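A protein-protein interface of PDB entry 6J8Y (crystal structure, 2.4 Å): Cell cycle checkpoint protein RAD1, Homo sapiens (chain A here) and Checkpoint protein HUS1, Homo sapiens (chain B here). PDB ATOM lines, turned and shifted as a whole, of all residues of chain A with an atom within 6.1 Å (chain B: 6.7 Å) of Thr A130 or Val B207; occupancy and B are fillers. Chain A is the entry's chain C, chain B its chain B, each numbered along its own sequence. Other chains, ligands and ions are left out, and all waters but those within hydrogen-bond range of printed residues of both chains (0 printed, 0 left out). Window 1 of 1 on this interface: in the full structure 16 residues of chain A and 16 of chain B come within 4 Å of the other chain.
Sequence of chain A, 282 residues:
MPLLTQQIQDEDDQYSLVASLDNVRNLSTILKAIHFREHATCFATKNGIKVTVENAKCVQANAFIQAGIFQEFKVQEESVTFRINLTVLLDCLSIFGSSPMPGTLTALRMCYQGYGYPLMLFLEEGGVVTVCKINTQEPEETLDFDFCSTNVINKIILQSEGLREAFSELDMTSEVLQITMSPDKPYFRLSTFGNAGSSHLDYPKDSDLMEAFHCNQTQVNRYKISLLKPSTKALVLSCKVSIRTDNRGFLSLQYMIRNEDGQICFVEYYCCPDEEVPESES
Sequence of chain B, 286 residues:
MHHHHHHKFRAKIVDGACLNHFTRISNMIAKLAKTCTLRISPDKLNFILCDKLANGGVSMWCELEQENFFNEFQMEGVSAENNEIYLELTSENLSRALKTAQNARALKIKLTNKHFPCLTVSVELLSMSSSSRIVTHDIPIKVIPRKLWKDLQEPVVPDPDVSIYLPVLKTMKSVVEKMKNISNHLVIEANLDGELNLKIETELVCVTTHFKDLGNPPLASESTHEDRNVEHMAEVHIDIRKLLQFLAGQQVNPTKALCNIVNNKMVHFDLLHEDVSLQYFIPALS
Of the printed residues of chain B, Ile A95 touches Val B175 (3.2 Å) and Met B179 (3.9 Å).
Phe A122 touches none of the printed residues of chain B.
Glu A124 touches none of the printed residues of chain B.
Thr A130 touches just these residues of chain B: Val B207 (3.7 Å), Thr B208 (3.3 Å) and Thr B209 (3.0 Å).
Printed residues of chain A within 4 Å of Val B175: Ile A95.
Of the printed residues of chain A, Val B205 touches Lys A133.
Printed residues of chain A within 4 Å of Thr B208: Val A129, Thr A130 and Val A131.
The nearest residue of chain B that does not touch Thr A130 is His B210 (4.6 Å).
The backbone carbonyl oxygen of Leu B198 is in hydrogen-bond range of the backbone NH of Thr B209 (2.9 Å).
The backbone NH (N) of Ile B200 lies within hydrogen-bond range of the backbone carbonyl oxygen (O) of Val B207 (3.1 Å).
The backbone carbonyl oxygen (O) of Val B205 lies within hydrogen-bond range of the side-chain hydroxyl (OG1) of Thr B202, 3.1 Å away.
The side-chain sulfur of Cys A92 lies close to the side-chain sulfur of Cys A132 (3.7 Å).
O of Leu A121 is in hydrogen-bond range of N of Cys A132 (2.8 Å).
O of Leu A123 lies within hydrogen-bond range of N of Thr A130, 2.8 Å away.
Of the 14 printed residues of chain B, 8 touch a printed residue of chain A.
Hydrophobic or aromatic side chains of chain B within 4 Å of the printed part of chain A: Val B175, Met B179, Val B205, Val B207 and His B210.
Hydrophobic or aromatic side chains of chain A that line the printed part of chain B: Ile A95, Val A128 and Val A131.
Among the printed residues, 17 pairs touch across the chains.
Among the printed residues, no Asp or Glu carboxylate lies within 4 Å of a Lys or Arg side-chain nitrogen of the other chain.
Val B207 touches Cys A92 (CG2 to SG, 3.98 Å).
Ile A95 touches Val B175.
Met B179 touches Ile A95 (CG to CD1, 3.9 Å).
Val A128 touches Thr B209.
Thr B208 touches Val A129 (O to O, 3.8 Å).
Val A129 touches Thr B209 (O to C, 3.5 Å).
O of Thr B208 touches CA of Thr A130, 3.3 Å away.
O of Cys B206 touches O of Val A131 (3.6 Å).
Val A131 touches Val B207.
Cys A132 touches Cys B206.
N of Lys A133 lies within hydrogen-bond range of O of Cys B206 (2.8 Å).
The backbone carbonyl oxygen of Thr B208 is in hydrogen-bond range of the backbone NH of Val A131 (2.7 Å).
The side-chain hydroxyl (OG1) of Thr A130 sits at hydrogen-bond distance from the side-chain hydroxyl (OG1) of Thr B209.
The backbone NH (N) of His B210 lies within hydrogen-bond range of the backbone carbonyl oxygen (O) of Val A129, at 2.6 Å.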
ATOM      1  N   CYS A  92      -7.475  -5.361   4.824  1.00  0.00           N
ATOM      2  CA  CYS A  92      -7.405  -6.797   5.063  1.00  0.00           C
ATOM      3  C   CYS A  92      -8.784  -7.446   4.984  1.00  0.00           C
ATOM      4  O   CYS A  92      -8.945  -8.503   4.373  1.00  0.00           O
ATOM      5  CB  CYS A  92      -6.773  -7.081   6.429  1.00  0.00           C
ATOM      6  SG  CYS A  92      -5.012  -6.680   6.540  1.00  0.00           S
ATOM      7  N   ILE A  95      -9.879  -8.041   1.421  1.00  0.00           N
ATOM      8  CA  ILE A  95      -8.746  -8.518   0.632  1.00  0.00           C
ATOM      9  C   ILE A  95      -9.181  -9.359  -0.569  1.00  0.00           C
ATOM     10  O   ILE A  95      -8.404  -9.569  -1.499  1.00  0.00           O
ATOM     11  CB  ILE A  95      -7.769  -9.344   1.507  1.00  0.00           C
ATOM     12  CG1 ILE A  95      -6.380  -9.408   0.865  1.00  0.00           C
ATOM     13  CG2 ILE A  95      -8.323 -10.736   1.779  1.00  0.00           C
ATOM     14  CD1 ILE A  95      -5.713  -8.059   0.718  1.00  0.00           C
ATOM     15  N   PHE A  96     -10.425  -9.830  -0.561  1.00  0.00           N
ATOM     16  CA  PHE A  96     -10.909 -10.673  -1.650  1.00  0.00           C
ATOM     17  C   PHE A  96     -11.789  -9.910  -2.637  1.00  0.00           C
ATOM     18  O   PHE A  96     -12.481 -10.516  -3.455  1.00  0.00           O
ATOM     19  CB  PHE A  96     -11.673 -11.878  -1.095  1.00  0.00           C
ATOM     20  CG  PHE A  96     -10.786 -12.949  -0.528  1.00  0.00           C
ATOM     21  CD1 PHE A  96     -10.024 -13.749  -1.364  1.00  0.00           C
ATOM     22  CD2 PHE A  96     -10.716 -13.160   0.840  1.00  0.00           C
ATOM     23  CE1 PHE A  96      -9.207 -14.736  -0.848  1.00  0.00           C
ATOM     24  CE2 PHE A  96      -9.900 -14.147   1.361  1.00  0.00           C
ATOM     25  CZ  PHE A  96      -9.146 -14.936   0.515  1.00  0.00           C
ATOM     26  N   LEU A 121      -6.426 -12.245  11.684  1.00  0.00           N
ATOM     27  CA  LEU A 121      -7.567 -12.307  10.780  1.00  0.00           C
ATOM     28  C   LEU A 121      -7.458 -13.489   9.827  1.00  0.00           C
ATOM     29  O   LEU A 121      -6.479 -13.619   9.092  1.00  0.00           O
ATOM     30  CB  LEU A 121      -7.695 -11.010   9.979  1.00  0.00           C
ATOM     31  CG  LEU A 121      -7.905  -9.712  10.756  1.00  0.00           C
ATOM     32  CD1 LEU A 121      -8.074  -8.553   9.790  1.00  0.00           C
ATOM     33  CD2 LEU A 121      -9.105  -9.825  11.683  1.00  0.00           C
ATOM     34  N   PHE A 122      -8.470 -14.349   9.844  1.00  0.00           N
ATOM     35  CA  PHE A 122      -8.521 -15.492   8.941  1.00  0.00           C
ATOM     36  C   PHE A 122      -9.697 -15.355   7.985  1.00  0.00           C
ATOM     37  O   PHE A 122     -10.836 -15.656   8.342  1.00  0.00           O
ATOM     38  CB  PHE A 122      -8.624 -16.801   9.725  1.00  0.00           C
ATOM     39  CG  PHE A 122      -7.426 -17.091  10.585  1.00  0.00           C
ATOM     40  CD1 PHE A 122      -7.297 -16.511  11.836  1.00  0.00           C
ATOM     41  CD2 PHE A 122      -6.431 -17.947  10.143  1.00  0.00           C
ATOM     42  CE1 PHE A 122      -6.196 -16.776  12.629  1.00  0.00           C
ATOM     43  CE2 PHE A 122      -5.328 -18.217  10.933  1.00  0.00           C
ATOM     44  CZ  PHE A 122      -5.210 -17.630  12.176  1.00  0.00           C
ATOM     45  N   LEU A 123      -9.418 -14.890   6.773  1.00  0.00           N
ATOM     46  CA  LEU A 123     -10.459 -14.704   5.771  1.00  0.00           C
ATOM     47  C   LEU A 123     -10.413 -15.811   4.727  1.00  0.00           C
ATOM     48  O   LEU A 123      -9.349 -16.147   4.210  1.00  0.00           O
ATOM     49  CB  LEU A 123     -10.323 -13.335   5.103  1.00  0.00           C
ATOM     50  CG  LEU A 123     -10.329 -12.133   6.051  1.00  0.00           C
ATOM     51  CD1 LEU A 123      -8.925 -11.581   6.239  1.00  0.00           C
ATOM     52  CD2 LEU A 123     -11.267 -11.055   5.545  1.00  0.00           C
ATOM     53  N   GLU A 124     -11.577 -16.376   4.422  1.00  0.00           N
ATOM     54  CA  GLU A 124     -11.668 -17.477   3.473  1.00  0.00           C
ATOM     55  C   GLU A 124     -12.694 -17.181   2.385  1.00  0.00           C
ATOM     56  O   GLU A 124     -13.762 -16.634   2.657  1.00  0.00           O
ATOM     57  CB  GLU A 124     -12.022 -18.779   4.204  1.00  0.00           C
ATOM     58  CG  GLU A 124     -12.063 -20.035   3.330  1.00  0.00           C
ATOM     59  CD  GLU A 124     -13.367 -20.198   2.568  1.00  0.00           C
ATOM     60  OE1 GLU A 124     -14.397 -19.650   3.019  1.00  0.00           O
ATOM     61  OE2 GLU A 124     -13.362 -20.871   1.514  1.00  0.00           O
ATOM     62  N   VAL A 128      -9.758 -20.457  -0.852  1.00  0.00           N
ATOM     63  CA  VAL A 128      -8.599 -19.580  -0.763  1.00  0.00           C
ATOM     64  C   VAL A 128      -8.581 -18.905   0.602  1.00  0.00           C
ATOM     65  O   VAL A 128      -9.570 -18.300   1.016  1.00  0.00           O
ATOM     66  CB  VAL A 128      -8.605 -18.509  -1.869  1.00  0.00           C
ATOM     67  CG1 VAL A 128      -7.315 -17.703  -1.829  1.00  0.00           C
ATOM     68  CG2 VAL A 128      -8.795 -19.154  -3.234  1.00  0.00           C
ATOM     69  N   VAL A 129      -7.458 -19.013   1.301  1.00  0.00           N
ATOM     70  CA  VAL A 129      -7.359 -18.472   2.650  1.00  0.00           C
ATOM     71  C   VAL A 129      -6.300 -17.382   2.754  1.00  0.00           C
ATOM     72  O   VAL A 129      -5.153 -17.573   2.352  1.00  0.00           O
ATOM     73  CB  VAL A 129      -7.037 -19.580   3.674  1.00  0.00           C
ATOM     74  CG1 VAL A 129      -6.870 -18.987   5.065  1.00  0.00           C
ATOM     75  CG2 VAL A 129      -8.125 -20.642   3.665  1.00  0.00           C
ATOM     76  N   THR A 130      -6.699 -16.235   3.294  1.00  0.00           N
ATOM     77  CA  THR A 130      -5.772 -15.144   3.558  1.00  0.00           C
ATOM     78  C   THR A 130      -5.601 -14.968   5.062  1.00  0.00           C
ATOM     79  O   THR A 130      -6.583 -14.890   5.801  1.00  0.00           O
ATOM     80  CB  THR A 130      -6.255 -13.823   2.930  1.00  0.00           C
ATOM     81  OG1 THR A 130      -6.370 -13.980   1.511  1.00  0.00           O
ATOM     82  CG2 THR A 130      -5.279 -12.697   3.233  1.00  0.00           C
ATOM     83  N   VAL A 131      -4.352 -14.912   5.513  1.00  0.00           N
ATOM     84  CA  VAL A 131      -4.055 -14.795   6.937  1.00  0.00           C
ATOM     85  C   VAL A 131      -3.379 -13.466   7.256  1.00  0.00           C
ATOM     86  O   VAL A 131      -2.275 -13.194   6.785  1.00  0.00           O
ATOM     87  CB  VAL A 131      -3.157 -15.948   7.416  1.00  0.00           C
ATOM     88  CG1 VAL A 131      -2.907 -15.840   8.910  1.00  0.00           C
ATOM     89  CG2 VAL A 131      -3.788 -17.289   7.070  1.00  0.00           C
ATOM     90  N   CYS A 132      -4.042 -12.645   8.065  1.00  0.00           N
ATOM     91  CA  CYS A 132      -3.537 -11.313   8.380  1.00  0.00           C
ATOM     92  C   CYS A 132      -3.097 -11.194   9.835  1.00  0.00           C
ATOM     93  O   CYS A 132      -3.791 -11.648  10.744  1.00  0.00           O
ATOM     94  CB  CYS A 132      -4.603 -10.258   8.075  1.00  0.00           C
ATOM     95  SG  CYS A 132      -5.312 -10.378   6.418  1.00  0.00           S
ATOM     96  N   LYS A 133      -1.939 -10.576  10.047  1.00  0.00           N
ATOM     97  CA  LYS A 133      -1.419 -10.350  11.390  1.00  0.00           C
ATOM     98  C   LYS A 133      -1.162  -8.864  11.612  1.00  0.00           C
ATOM     99  O   LYS A 133      -0.138  -8.334  11.185  1.00  0.00           O
ATOM    100  CB  LYS A 133      -0.137 -11.154  11.615  1.00  0.00           C
ATOM    101  CG  LYS A 133      -0.244 -12.606  11.182  1.00  0.00           C
ATOM    102  CD  LYS A 133       0.657 -13.515  12.002  1.00  0.00           C
ATOM    103  CE  LYS A 133       0.812 -14.875  11.336  1.00  0.00           C
ATOM    104  NZ  LYS A 133       1.244 -15.924  12.301  1.00  0.00           N
ATOM    105  N   VAL B 175      -6.827  -9.697  -4.683  1.00  0.00           N
ATOM    106  CA  VAL B 175      -5.937  -9.835  -3.536  1.00  0.00           C
ATOM    107  C   VAL B 175      -4.707  -8.938  -3.670  1.00  0.00           C
ATOM    108  O   VAL B 175      -4.421  -8.136  -2.783  1.00  0.00           O
ATOM    109  CB  VAL B 175      -5.487 -11.297  -3.344  1.00  0.00           C
ATOM    110  CG1 VAL B 175      -4.355 -11.379  -2.339  1.00  0.00           C
ATOM    111  CG2 VAL B 175      -6.658 -12.157  -2.894  1.00  0.00           C
ATOM    112  N   MET B 179      -3.512  -5.577  -1.624  1.00  0.00           N
ATOM    113  CA  MET B 179      -2.216  -5.712  -0.964  1.00  0.00           C
ATOM    114  C   MET B 179      -1.320  -4.527  -1.314  1.00  0.00           C
ATOM    115  O   MET B 179      -0.425  -4.164  -0.549  1.00  0.00           O
ATOM    116  CB  MET B 179      -1.527  -7.023  -1.354  1.00  0.00           C
ATOM    117  CG  MET B 179      -2.110  -8.270  -0.702  1.00  0.00           C
ATOM    118  SD  MET B 179      -1.397  -9.802  -1.344  1.00  0.00           S
ATOM    119  CE  MET B 179      -0.150 -10.163  -0.114  1.00  0.00           C
ATOM    120  N   ILE B 182      -1.132  -1.825   1.197  1.00  0.00           N
ATOM    121  CA  ILE B 182      -0.303  -2.119   2.360  1.00  0.00           C
ATOM    122  C   ILE B 182       1.182  -1.963   2.050  1.00  0.00           C
ATOM    123  O   ILE B 182       1.920  -1.333   2.807  1.00  0.00           O
ATOM    124  CB  ILE B 182      -0.555  -3.546   2.881  1.00  0.00           C
ATOM    125  CG1 ILE B 182      -2.050  -3.779   3.108  1.00  0.00           C
ATOM    126  CG2 ILE B 182       0.237  -3.797   4.155  1.00  0.00           C
ATOM    127  CD1 ILE B 182      -2.638  -2.933   4.213  1.00  0.00           C
ATOM    128  N   LEU B 198       0.875 -15.712  -1.922  1.00  0.00           N
ATOM    129  CA  LEU B 198       1.201 -14.305  -2.116  1.00  0.00           C
ATOM    130  C   LEU B 198       1.436 -13.687  -0.745  1.00  0.00           C
ATOM    131  O   LEU B 198       0.643 -13.894   0.174  1.00  0.00           O
ATOM    132  CB  LEU B 198       0.083 -13.579  -2.864  1.00  0.00           C
ATOM    133  CG  LEU B 198      -0.251 -14.143  -4.246  1.00  0.00           C
ATOM    134  CD1 LEU B 198      -1.410 -13.383  -4.871  1.00  0.00           C
ATOM    135  CD2 LEU B 198       0.972 -14.105  -5.149  1.00  0.00           C
ATOM    136  N   LYS B 199       2.522 -12.935  -0.598  1.00  0.00           N
ATOM    137  CA  LYS B 199       2.972 -12.556   0.735  1.00  0.00           C
ATOM    138  C   LYS B 199       3.613 -11.173   0.811  1.00  0.00           C
ATOM    139  O   LYS B 199       4.630 -10.908   0.169  1.00  0.00           O
ATOM    140  CB  LYS B 199       3.954 -13.612   1.247  1.00  0.00           C
ATOM    141  CG  LYS B 199       4.261 -13.540   2.731  1.00  0.00           C
ATOM    142  CD  LYS B 199       4.643 -14.915   3.266  1.00  0.00           C
ATOM    143  CE  LYS B 199       5.639 -15.612   2.349  1.00  0.00           C
ATOM    144  NZ  LYS B 199       5.982 -16.978   2.833  1.00  0.00           N
ATOM    145  N   ILE B 200       3.005 -10.294   1.602  1.00  0.00           N
ATOM    146  CA  ILE B 200       3.605  -9.008   1.935  1.00  0.00           C
ATOM    147  C   ILE B 200       3.911  -8.978   3.426  1.00  0.00           C
ATOM    148  O   ILE B 200       3.236  -9.638   4.218  1.00  0.00           O
ATOM    149  CB  ILE B 200       2.692  -7.821   1.568  1.00  0.00           C
ATOM    150  CG1 ILE B 200       1.337  -7.953   2.266  1.00  0.00           C
ATOM    151  CG2 ILE B 200       2.517  -7.723   0.060  1.00  0.00           C
ATOM    152  CD1 ILE B 200       0.328  -6.913   1.842  1.00  0.00           C
ATOM    153  N   GLU B 201       4.928  -8.217   3.810  1.00  0.00           N
ATOM    154  CA  GLU B 201       5.365  -8.192   5.199  1.00  0.00           C
ATOM    155  C   GLU B 201       5.964  -6.844   5.576  1.00  0.00           C
ATOM    156  O   GLU B 201       6.977  -6.425   5.016  1.00  0.00           O
ATOM    157  CB  GLU B 201       6.383  -9.306   5.451  1.00  0.00           C
ATOM    158  CG  GLU B 201       6.770  -9.483   6.909  1.00  0.00           C
ATOM    159  CD  GLU B 201       7.612 -10.724   7.136  1.00  0.00           C
ATOM    160  OE1 GLU B 201       8.045 -11.340   6.139  1.00  0.00           O
ATOM    161  OE2 GLU B 201       7.839 -11.083   8.311  1.00  0.00           O
ATOM    162  N   THR B 202       5.327  -6.163   6.522  1.00  0.00           N
ATOM    163  CA  THR B 202       5.836  -4.889   7.010  1.00  0.00           C
ATOM    164  C   THR B 202       6.020  -4.917   8.523  1.00  0.00           C
ATOM    165  O   THR B 202       5.754  -5.925   9.180  1.00  0.00           O
ATOM    166  CB  THR B 202       4.903  -3.715   6.642  1.00  0.00           C
ATOM    167  OG1 THR B 202       3.741  -3.738   7.480  1.00  0.00           O
ATOM    168  CG2 THR B 202       4.481  -3.793   5.181  1.00  0.00           C
ATOM    169  N   VAL B 205       2.202  -5.080   9.958  1.00  0.00           N
ATOM    170  CA  VAL B 205       1.203  -5.998   9.420  1.00  0.00           C
ATOM    171  C   VAL B 205       1.799  -7.000   8.431  1.00  0.00           C
ATOM    172  O   VAL B 205       2.557  -6.633   7.533  1.00  0.00           O
ATOM    173  CB  VAL B 205       0.046  -5.225   8.736  1.00  0.00           C
ATOM    174  CG1 VAL B 205       0.588  -4.163   7.790  1.00  0.00           C
ATOM    175  CG2 VAL B 205      -0.895  -6.180   8.011  1.00  0.00           C
ATOM    176  N   CYS B 206       1.458  -8.272   8.618  1.00  0.00           N
ATOM    177  CA  CYS B 206       1.866  -9.331   7.703  1.00  0.00           C
ATOM    178  C   CYS B 206       0.637  -9.981   7.080  1.00  0.00           C
ATOM    179  O   CYS B 206      -0.302 -10.349   7.785  1.00  0.00           O
ATOM    180  CB  CYS B 206       2.712 -10.379   8.429  1.00  0.00           C
ATOM    181  SG  CYS B 206       4.068  -9.700   9.414  1.00  0.00           S
ATOM    182  N   VAL B 207       0.637 -10.114   5.757  1.00  0.00           N
ATOM    183  CA  VAL B 207      -0.500 -10.702   5.054  1.00  0.00           C
ATOM    184  C   VAL B 207      -0.060 -11.815   4.107  1.00  0.00           C
ATOM    185  O   VAL B 207       0.808 -11.614   3.259  1.00  0.00           O
ATOM    186  CB  VAL B 207      -1.279  -9.640   4.250  1.00  0.00           C
ATOM    187  CG1 VAL B 207      -2.449 -10.281   3.520  1.00  0.00           C
ATOM    188  CG2 VAL B 207      -1.764  -8.522   5.162  1.00  0.00           C
ATOM    189  N   THR B 208      -0.668 -12.989   4.256  1.00  0.00           N
ATOM    190  CA  THR B 208      -0.357 -14.127   3.401  1.00  0.00           C
ATOM    191  C   THR B 208      -1.625 -14.765   2.840  1.00  0.00           C
ATOM    192  O   THR B 208      -2.501 -15.186   3.591  1.00  0.00           O
ATOM    193  CB  THR B 208       0.449 -15.202   4.157  1.00  0.00           C
ATOM    194  OG1 THR B 208       1.671 -14.636   4.645  1.00  0.00           O
ATOM    195  CG2 THR B 208       0.771 -16.368   3.238  1.00  0.00           C
ATOM    196  N   THR B 209      -1.713 -14.831   1.516  1.00  0.00           N
ATOM    197  CA  THR B 209      -2.849 -15.460   0.854  1.00  0.00           C
ATOM    198  C   THR B 209      -2.457 -16.833   0.317  1.00  0.00           C
ATOM    199  O   THR B 209      -1.499 -16.959  -0.446  1.00  0.00           O
ATOM    200  CB  THR B 209      -3.385 -14.592  -0.299  1.00  0.00           C
ATOM    201  OG1 THR B 209      -3.782 -13.313   0.209  1.00  0.00           O
ATOM    202  CG2 THR B 209      -4.579 -15.259  -0.960  1.00  0.00           C
ATOM    203  N   HIS B 210      -3.199 -17.860   0.718  1.00  0.00           N
ATOM    204  CA  HIS B 210      -2.865 -19.233   0.353  1.00  0.00           C
ATOM    205  C   HIS B 210      -3.760 -19.796  -0.747  1.00  0.00           C
ATOM    206  O   HIS B 210      -4.980 -19.854  -0.601  1.00  0.00           O
ATOM    207  CB  HIS B 210      -2.944 -20.142   1.583  1.00  0.00           C
ATOM    208  CG  HIS B 210      -1.992 -19.768   2.676  1.00  0.00           C
ATOM    209  ND1 HIS B 210      -0.725 -20.302   2.773  1.00  0.00           N
ATOM    210  CD2 HIS B 210      -2.125 -18.921   3.724  1.00  0.00           C
ATOM    211  CE1 HIS B 210      -0.116 -19.796   3.832  1.00  0.00           C
ATOM    212  NE2 HIS B 210      -0.944 -18.956   4.426  1.00  0.00           N
